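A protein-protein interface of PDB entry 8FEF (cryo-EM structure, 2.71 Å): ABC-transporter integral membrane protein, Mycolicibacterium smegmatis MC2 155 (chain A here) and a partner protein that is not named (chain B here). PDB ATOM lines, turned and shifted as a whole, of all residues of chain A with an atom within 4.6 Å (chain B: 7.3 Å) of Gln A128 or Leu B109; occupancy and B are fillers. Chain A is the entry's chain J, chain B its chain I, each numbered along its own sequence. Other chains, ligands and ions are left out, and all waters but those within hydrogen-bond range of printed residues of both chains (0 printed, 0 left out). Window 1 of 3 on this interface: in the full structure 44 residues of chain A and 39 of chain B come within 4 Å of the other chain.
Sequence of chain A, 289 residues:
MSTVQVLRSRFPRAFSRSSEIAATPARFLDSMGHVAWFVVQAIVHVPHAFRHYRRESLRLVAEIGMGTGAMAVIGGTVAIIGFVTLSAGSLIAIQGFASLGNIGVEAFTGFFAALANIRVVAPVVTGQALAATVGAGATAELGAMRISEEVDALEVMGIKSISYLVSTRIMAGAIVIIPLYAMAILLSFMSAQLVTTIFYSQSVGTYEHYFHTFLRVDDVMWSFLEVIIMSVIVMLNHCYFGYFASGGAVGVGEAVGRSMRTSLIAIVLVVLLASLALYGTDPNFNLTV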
ATOM      1  N   VAL A 124      22.884  17.058 -33.372  1.00  0.00           N
ATOM      2  CA  VAL A 124      22.690  18.253 -32.554  1.00  0.00           C
ATOM      3  C   VAL A 124      21.493  18.082 -31.624  1.00  0.00           C
ATOM      4  O   VAL A 124      21.563  18.401 -30.434  1.00  0.00           O
ATOM      5  CB  VAL A 124      22.532  19.494 -33.451  1.00  0.00           C
ATOM      6  CG1 VAL A 124      22.156  20.708 -32.622  1.00  0.00           C
ATOM      7  CG2 VAL A 124      23.811  19.756 -34.219  1.00  0.00           C
ATOM      8  N   VAL A 125      20.382  17.569 -32.153  1.00  0.00           N
ATOM      9  CA  VAL A 125      19.163  17.433 -31.358  1.00  0.00           C
ATOM     10  C   VAL A 125      19.354  16.412 -30.239  1.00  0.00           C
ATOM     11  O   VAL A 125      18.971  16.652 -29.084  1.00  0.00           O
ATOM     12  CB  VAL A 125      17.982  17.070 -32.277  1.00  0.00           C
ATOM     13  CG1 VAL A 125      16.929  16.285 -31.533  1.00  0.00           C
ATOM     14  CG2 VAL A 125      17.380  18.331 -32.872  1.00  0.00           C
ATOM     15  N   THR A 126      19.954  15.262 -30.561  1.00  0.00           N
ATOM     16  CA  THR A 126      20.258  14.272 -29.536  1.00  0.00           C
ATOM     17  C   THR A 126      21.222  14.836 -28.506  1.00  0.00           C
ATOM     18  O   THR A 126      21.098  14.555 -27.311  1.00  0.00           O
ATOM     19  CB  THR A 126      20.836  13.013 -30.182  1.00  0.00           C
ATOM     20  OG1 THR A 126      19.929  12.532 -31.181  1.00  0.00           O
ATOM     21  CG2 THR A 126      21.060  11.925 -29.142  1.00  0.00           C
ATOM     22  N   GLY A 127      22.179  15.652 -28.950  1.00  0.00           N
ATOM     23  CA  GLY A 127      23.092  16.277 -28.015  1.00  0.00           C
ATOM     24  C   GLY A 127      22.398  17.214 -27.052  1.00  0.00           C
ATOM     25  O   GLY A 127      22.683  17.201 -25.858  1.00  0.00           O
ATOM     26  N   GLN A 128      21.480  18.042 -27.555  1.00  0.00           N
ATOM     27  CA  GLN A 128      20.777  18.969 -26.670  1.00  0.00           C
ATOM     28  C   GLN A 128      19.884  18.224 -25.685  1.00  0.00           C
ATOM     29  O   GLN A 128      19.820  18.587 -24.504  1.00  0.00           O
ATOM     30  CB  GLN A 128      19.958  19.983 -27.474  1.00  0.00           C
ATOM     31  CG  GLN A 128      20.672  20.684 -28.640  1.00  0.00           C
ATOM     32  CD  GLN A 128      21.813  21.620 -28.242  1.00  0.00           C
ATOM     33  OE1 GLN A 128      22.607  21.330 -27.349  1.00  0.00           O
ATOM     34  NE2 GLN A 128      21.903  22.752 -28.929  1.00  0.00           N
ATOM     35  N   ALA A 129      19.183  17.185 -26.149  1.00  0.00           N
ATOM     36  CA  ALA A 129      18.336  16.413 -25.240  1.00  0.00           C
ATOM     37  C   ALA A 129      19.165  15.677 -24.191  1.00  0.00           C
ATOM     38  O   ALA A 129      18.792  15.638 -23.008  1.00  0.00           O
ATOM     39  CB  ALA A 129      17.472  15.437 -26.034  1.00  0.00           C
ATOM     40  N   LEU A 130      20.289  15.086 -24.605  1.00  0.00           N
ATOM     41  CA  LEU A 130      21.195  14.431 -23.668  1.00  0.00           C
ATOM     42  C   LEU A 130      21.758  15.429 -22.669  1.00  0.00           C
ATOM     43  O   LEU A 130      21.805  15.155 -21.465  1.00  0.00           O
ATOM     44  CB  LEU A 130      22.326  13.744 -24.433  1.00  0.00           C
ATOM     45  CG  LEU A 130      23.549  13.316 -23.622  1.00  0.00           C
ATOM     46  CD1 LEU A 130      23.313  11.976 -22.947  1.00  0.00           C
ATOM     47  CD2 LEU A 130      24.784  13.272 -24.501  1.00  0.00           C
ATOM     48  N   ALA A 131      22.193  16.594 -23.159  1.00  0.00           N
ATOM     49  CA  ALA A 131      22.646  17.676 -22.298  1.00  0.00           C
ATOM     50  C   ALA A 131      21.611  17.965 -21.229  1.00  0.00           C
ATOM     51  O   ALA A 131      21.871  17.758 -20.043  1.00  0.00           O
ATOM     52  CB  ALA A 131      22.936  18.927 -23.128  1.00  0.00           C
ATOM     53  N   ALA A 132      20.403  18.355 -21.649  1.00  0.00           N
ATOM     54  CA  ALA A 132      19.319  18.667 -20.726  1.00  0.00           C
ATOM     55  C   ALA A 132      19.169  17.567 -19.687  1.00  0.00           C
ATOM     56  O   ALA A 132      19.581  17.755 -18.537  1.00  0.00           O
ATOM     57  CB  ALA A 132      18.005  18.861 -21.484  1.00  0.00           C
ATOM     58  N   SER A 263      26.792  23.777 -22.421  1.00  0.00           N
ATOM     59  CA  SER A 263      26.604  22.526 -23.145  1.00  0.00           C
ATOM     60  C   SER A 263      26.033  22.764 -24.534  1.00  0.00           C
ATOM     61  O   SER A 263      26.472  22.135 -25.503  1.00  0.00           O
ATOM     62  CB  SER A 263      25.693  21.595 -22.349  1.00  0.00           C
ATOM     63  OG  SER A 263      26.226  21.358 -21.062  1.00  0.00           O
ATOM     64  N   LEU A 264      25.042  23.655 -24.652  1.00  0.00           N
ATOM     65  CA  LEU A 264      24.497  23.975 -25.971  1.00  0.00           C
ATOM     66  C   LEU A 264      25.595  24.479 -26.898  1.00  0.00           C
ATOM     67  O   LEU A 264      25.743  24.001 -28.039  1.00  0.00           O
ATOM     68  CB  LEU A 264      23.386  25.022 -25.856  1.00  0.00           C
ATOM     69  CG  LEU A 264      22.148  24.785 -24.986  1.00  0.00           C
ATOM     70  CD1 LEU A 264      21.262  26.020 -24.991  1.00  0.00           C
ATOM     71  CD2 LEU A 264      21.365  23.566 -25.425  1.00  0.00           C
ATOM     72  N   ILE A 267      28.104  21.622 -27.859  1.00  0.00           N
ATOM     73  CA  ILE A 267      27.543  20.628 -28.773  1.00  0.00           C
ATOM     74  C   ILE A 267      27.514  21.166 -30.196  1.00  0.00           C
ATOM     75  O   ILE A 267      27.947  20.493 -31.147  1.00  0.00           O
ATOM     76  CB  ILE A 267      26.138  20.206 -28.311  1.00  0.00           C
ATOM     77  CG1 ILE A 267      26.228  19.387 -27.030  1.00  0.00           C
ATOM     78  CG2 ILE A 267      25.419  19.430 -29.401  1.00  0.00           C
ATOM     79  CD1 ILE A 267      24.959  19.374 -26.240  1.00  0.00           C
ATOM     80  N   VAL A 268      26.997  22.388 -30.364  1.00  0.00           N
ATOM     81  CA  VAL A 268      26.903  22.944 -31.713  1.00  0.00           C
ATOM     82  C   VAL A 268      28.293  23.110 -32.317  1.00  0.00           C
ATOM     83  O   VAL A 268      28.518  22.790 -33.494  1.00  0.00           O
ATOM     84  CB  VAL A 268      26.113  24.265 -31.700  1.00  0.00           C
ATOM     85  CG1 VAL A 268      26.026  24.833 -33.097  1.00  0.00           C
ATOM     86  CG2 VAL A 268      24.721  24.032 -31.149  1.00  0.00           C
ATOM     87  N   VAL B  65      25.202  30.043 -30.299  1.00  0.00           N
ATOM     88  CA  VAL B  65      24.592  28.812 -30.793  1.00  0.00           C
ATOM     89  C   VAL B  65      24.070  29.010 -32.213  1.00  0.00           C
ATOM     90  O   VAL B  65      24.100  28.084 -33.029  1.00  0.00           O
ATOM     91  CB  VAL B  65      23.473  28.339 -29.844  1.00  0.00           C
ATOM     92  CG1 VAL B  65      22.730  27.143 -30.416  1.00  0.00           C
ATOM     93  CG2 VAL B  65      24.054  27.979 -28.489  1.00  0.00           C
ATOM     94  N   LEU B  69      25.592  27.001 -35.923  1.00  0.00           N
ATOM     95  CA  LEU B  69      24.532  26.146 -36.450  1.00  0.00           C
ATOM     96  C   LEU B  69      24.132  26.560 -37.861  1.00  0.00           C
ATOM     97  O   LEU B  69      23.981  25.706 -38.746  1.00  0.00           O
ATOM     98  CB  LEU B  69      23.322  26.178 -35.518  1.00  0.00           C
ATOM     99  CG  LEU B  69      22.208  25.174 -35.813  1.00  0.00           C
ATOM    100  CD1 LEU B  69      22.754  23.760 -35.823  1.00  0.00           C
ATOM    101  CD2 LEU B  69      21.093  25.307 -34.793  1.00  0.00           C
ATOM    102  N   GLY B 103      15.427  29.828 -36.533  1.00  0.00           N
ATOM    103  CA  GLY B 103      15.099  30.920 -35.648  1.00  0.00           C
ATOM    104  C   GLY B 103      14.348  30.467 -34.413  1.00  0.00           C
ATOM    105  O   GLY B 103      14.829  30.603 -33.281  1.00  0.00           O
ATOM    106  N   PRO B 104      13.135  29.938 -34.608  1.00  0.00           N
ATOM    107  CA  PRO B 104      12.354  29.454 -33.458  1.00  0.00           C
ATOM    108  C   PRO B 104      13.026  28.343 -32.666  1.00  0.00           C
ATOM    109  O   PRO B 104      12.847  28.291 -31.447  1.00  0.00           O
ATOM    110  CB  PRO B 104      11.047  28.980 -34.106  1.00  0.00           C
ATOM    111  CG  PRO B 104      10.922  29.813 -35.321  1.00  0.00           C
ATOM    112  CD  PRO B 104      12.319  29.986 -35.835  1.00  0.00           C
ATOM    113  N   LEU B 105      13.793  27.452 -33.298  1.00  0.00           N
ATOM    114  CA  LEU B 105      14.400  26.366 -32.529  1.00  0.00           C
ATOM    115  C   LEU B 105      15.584  26.845 -31.696  1.00  0.00           C
ATOM    116  O   LEU B 105      15.760  26.396 -30.556  1.00  0.00           O
ATOM    117  CB  LEU B 105      14.823  25.221 -33.447  1.00  0.00           C
ATOM    118  CG  LEU B 105      13.712  24.203 -33.694  1.00  0.00           C
ATOM    119  CD1 LEU B 105      14.242  23.019 -34.474  1.00  0.00           C
ATOM    120  CD2 LEU B 105      13.106  23.751 -32.375  1.00  0.00           C
ATOM    121  N   VAL B 106      16.417  27.733 -32.241  1.00  0.00           N
ATOM    122  CA  VAL B 106      17.463  28.337 -31.421  1.00  0.00           C
ATOM    123  C   VAL B 106      16.835  29.162 -30.306  1.00  0.00           C
ATOM    124  O   VAL B 106      17.343  29.199 -29.177  1.00  0.00           O
ATOM    125  CB  VAL B 106      18.420  29.171 -32.295  1.00  0.00           C
ATOM    126  CG1 VAL B 106      19.369  29.989 -31.435  1.00  0.00           C
ATOM    127  CG2 VAL B 106      19.219  28.259 -33.205  1.00  0.00           C
ATOM    128  N   THR B 107      15.702  29.811 -30.592  1.00  0.00           N
ATOM    129  CA  THR B 107      14.962  30.496 -29.538  1.00  0.00           C
ATOM    130  C   THR B 107      14.520  29.517 -28.457  1.00  0.00           C
ATOM    131  O   THR B 107      14.676  29.791 -27.265  1.00  0.00           O
ATOM    132  CB  THR B 107      13.756  31.223 -30.136  1.00  0.00           C
ATOM    133  OG1 THR B 107      14.212  32.255 -31.019  1.00  0.00           O
ATOM    134  CG2 THR B 107      12.903  31.841 -29.040  1.00  0.00           C
ATOM    135  N   VAL B 108      13.999  28.353 -28.861  1.00  0.00           N
ATOM    136  CA  VAL B 108      13.589  27.324 -27.906  1.00  0.00           C
ATOM    137  C   VAL B 108      14.757  26.927 -27.021  1.00  0.00           C
ATOM    138  O   VAL B 108      14.659  26.935 -25.787  1.00  0.00           O
ATOM    139  CB  VAL B 108      13.026  26.096 -28.648  1.00  0.00           C
ATOM    140  CG1 VAL B 108      13.048  24.865 -27.750  1.00  0.00           C
ATOM    141  CG2 VAL B 108      11.631  26.356 -29.128  1.00  0.00           C
ATOM    142  N   LEU B 109      15.890  26.596 -27.641  1.00  0.00           N
ATOM    143  CA  LEU B 109      17.039  26.110 -26.890  1.00  0.00           C
ATOM    144  C   LEU B 109      17.539  27.162 -25.907  1.00  0.00           C
ATOM    145  O   LEU B 109      17.607  26.916 -24.699  1.00  0.00           O
ATOM    146  CB  LEU B 109      18.151  25.693 -27.852  1.00  0.00           C
ATOM    147  CG  LEU B 109      17.814  24.519 -28.771  1.00  0.00           C
ATOM    148  CD1 LEU B 109      18.992  24.182 -29.666  1.00  0.00           C
ATOM    149  CD2 LEU B 109      17.393  23.310 -27.953  1.00  0.00           C
ATOM    150  N   VAL B 110      17.850  28.365 -26.403  1.00  0.00           N
ATOM    151  CA  VAL B 110      18.496  29.365 -25.554  1.00  0.00           C
ATOM    152  C   VAL B 110      17.502  30.131 -24.696  1.00  0.00           C
ATOM    153  O   VAL B 110      17.913  30.950 -23.864  1.00  0.00           O
ATOM    154  CB  VAL B 110      19.359  30.298 -26.429  1.00  0.00           C
ATOM    155  CG1 VAL B 110      20.423  30.992 -25.595  1.00  0.00           C
ATOM    156  CG2 VAL B 110      20.029  29.505 -27.533  1.00  0.00           C
ATOM    157  N   VAL B 111      16.205  29.871 -24.834  1.00  0.00           N
ATOM    158  CA  VAL B 111      15.238  30.403 -23.884  1.00  0.00           C
ATOM    159  C   VAL B 111      14.946  29.395 -22.785  1.00  0.00           C
ATOM    160  O   VAL B 111      15.073  29.719 -21.605  1.00  0.00           O
ATOM    161  CB  VAL B 111      13.952  30.847 -24.616  1.00  0.00           C
ATOM    162  CG1 VAL B 111      12.788  30.922 -23.648  1.00  0.00           C
ATOM    163  CG2 VAL B 111      14.168  32.208 -25.262  1.00  0.00           C
ATOM    164  N   ALA B 112      14.608  28.154 -23.151  1.00  0.00           N
ATOM    165  CA  ALA B 112      14.359  27.127 -22.147  1.00  0.00           C
ATOM    166  C   ALA B 112      15.593  26.873 -21.290  1.00  0.00           C
ATOM    167  O   ALA B 112      15.483  26.725 -20.067  1.00  0.00           O
ATOM    168  CB  ALA B 112      13.902  25.836 -22.824  1.00  0.00           C
ATOM    169  N   GLY B 113      16.776  26.812 -21.906  1.00  0.00           N
ATOM    170  CA  GLY B 113      17.980  26.532 -21.142  1.00  0.00           C
ATOM    171  C   GLY B 113      18.369  27.656 -20.203  1.00  0.00           C
ATOM    172  O   GLY B 113      18.790  27.409 -19.071  1.00  0.00           O
ATOM    173  N   ALA B 114      18.245  28.904 -20.656  1.00  0.00           N
ATOM    174  CA  ALA B 114      18.736  30.040 -19.883  1.00  0.00           C
ATOM    175  C   ALA B 114      17.629  30.768 -19.127  1.00  0.00           C
ATOM    176  O   ALA B 114      17.632  30.787 -17.894  1.00  0.00           O
ATOM    177  CB  ALA B 114      19.472  31.013 -20.811  1.00  0.00           C
ATOM    178  N   GLY B 115      16.652  31.323 -19.840  1.00  0.00           N
ATOM    179  CA  GLY B 115      15.688  32.203 -19.213  1.00  0.00           C
ATOM    180  C   GLY B 115      14.659  31.478 -18.376  1.00  0.00           C
ATOM    181  O   GLY B 115      14.335  31.919 -17.270  1.00  0.00           O
ATOM    182  N   LEU B 241      13.472  22.603 -17.306  1.00  0.00           N
ATOM    183  CA  LEU B 241      14.166  22.521 -18.586  1.00  0.00           C
ATOM    184  C   LEU B 241      13.624  21.382 -19.444  1.00  0.00           C
ATOM    185  O   LEU B 241      13.372  21.559 -20.644  1.00  0.00           O
ATOM    186  CB  LEU B 241      15.659  22.350 -18.330  1.00  0.00           C
ATOM    187  CG  LEU B 241      16.552  21.957 -19.492  1.00  0.00           C
ATOM    188  CD1 LEU B 241      16.755  23.121 -20.440  1.00  0.00           C
ATOM    189  CD2 LEU B 241      17.856  21.492 -18.914  1.00  0.00           C
ATOM    190  N   VAL B 245      11.606  21.846 -22.996  1.00  0.00           N
ATOM    191  CA  VAL B 245      12.102  21.276 -24.249  1.00  0.00           C
ATOM    192  C   VAL B 245      11.019  20.431 -24.914  1.00  0.00           C
ATOM    193  O   VAL B 245      10.730  20.590 -26.109  1.00  0.00           O
ATOM    194  CB  VAL B 245      13.386  20.465 -24.003  1.00  0.00           C
ATOM    195  CG1 VAL B 245      13.725  19.626 -25.219  1.00  0.00           C
ATOM    196  CG2 VAL B 245      14.539  21.398 -23.677  1.00  0.00           C
ATOM    197  N   LEU B 248       7.921  22.664 -26.087  1.00  0.00           N
ATOM    198  CA  LEU B 248       8.244  23.530 -27.213  1.00  0.00           C
ATOM    199  C   LEU B 248       8.473  22.727 -28.486  1.00  0.00           C
ATOM    200  O   LEU B 248       8.103  23.179 -29.572  1.00  0.00           O
ATOM    201  CB  LEU B 248       9.452  24.408 -26.885  1.00  0.00           C
ATOM    202  CG  LEU B 248       9.247  25.417 -25.746  1.00  0.00           C
ATOM    203  CD1 LEU B 248      10.396  26.409 -25.656  1.00  0.00           C
ATOM    204  CD2 LEU B 248       7.913  26.132 -25.857  1.00  0.00           C
ATOM    205  N   PHE B 249       9.060  21.529 -28.382  1.00  0.00           N
ATOM    206  CA  PHE B 249       9.192  20.698 -29.578  1.00  0.00           C
ATOM    207  C   PHE B 249       7.830  20.262 -30.112  1.00  0.00           C
ATOM    208  O   PHE B 249       7.599  20.288 -31.331  1.00  0.00           O
ATOM    209  CB  PHE B 249      10.080  19.489 -29.292  1.00  0.00           C
ATOM    210  CG  PHE B 249      11.520  19.701 -29.662  1.00  0.00           C
ATOM    211  CD1 PHE B 249      12.403  20.288 -28.772  1.00  0.00           C
ATOM    212  CD2 PHE B 249      11.989  19.323 -30.907  1.00  0.00           C
ATOM    213  CE1 PHE B 249      13.724  20.488 -29.114  1.00  0.00           C
ATOM    214  CE2 PHE B 249      13.309  19.522 -31.254  1.00  0.00           C
ATOM    215  CZ  PHE B 249      14.178  20.105 -30.357  1.00  0.00           C
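NE2 of Gln A128 touches CD1 of Leu B109, at 3.3 Å.
Ala A132 touches Leu B241 (CA to CD2, 3.7 Å).
Leu B109 touches Leu A264.
Val B65 touches Val A268 (CG1 to CG2, 3.8 Å).
Val A268 touches Leu B69.
Gln A128 touches one residue of chain B.
Of chain A, only Gln A128 and Leu A264 come within 4 Å of Leu B109.
Printed residues of chain A within 4 Å of Leu B241: Ala A132.
Of the printed residues of chain B, Ala A132 touches Leu B241.
Gly B103 touches none of the printed residues of chain A.
The nearest residue of chain B that does not touch Gln A128 is Val B65 (4.7 Å).
The nearest printed residue of chain A that does not touch Leu B109 is Val A124 (5.6 Å).
Printed residues of chain B that touch a printed residue of chain A: Val B65, Leu B69, Leu B109 and Leu B241.
Hydrophobic or aromatic side chains of chain B that line the printed part of chain A: Val B65, Leu B69, Leu B109 and Leu B241.
Along chain B the printed residues that touch a printed residue of chain A span positions 65 to 241.
Of the 13 printed residues of chain A, 4 touch a printed residue of chain B.
Among the printed residues, no Asp or Glu carboxylate lies within 4 Å of a Lys or Arg side-chain nitrogen of the other chain.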
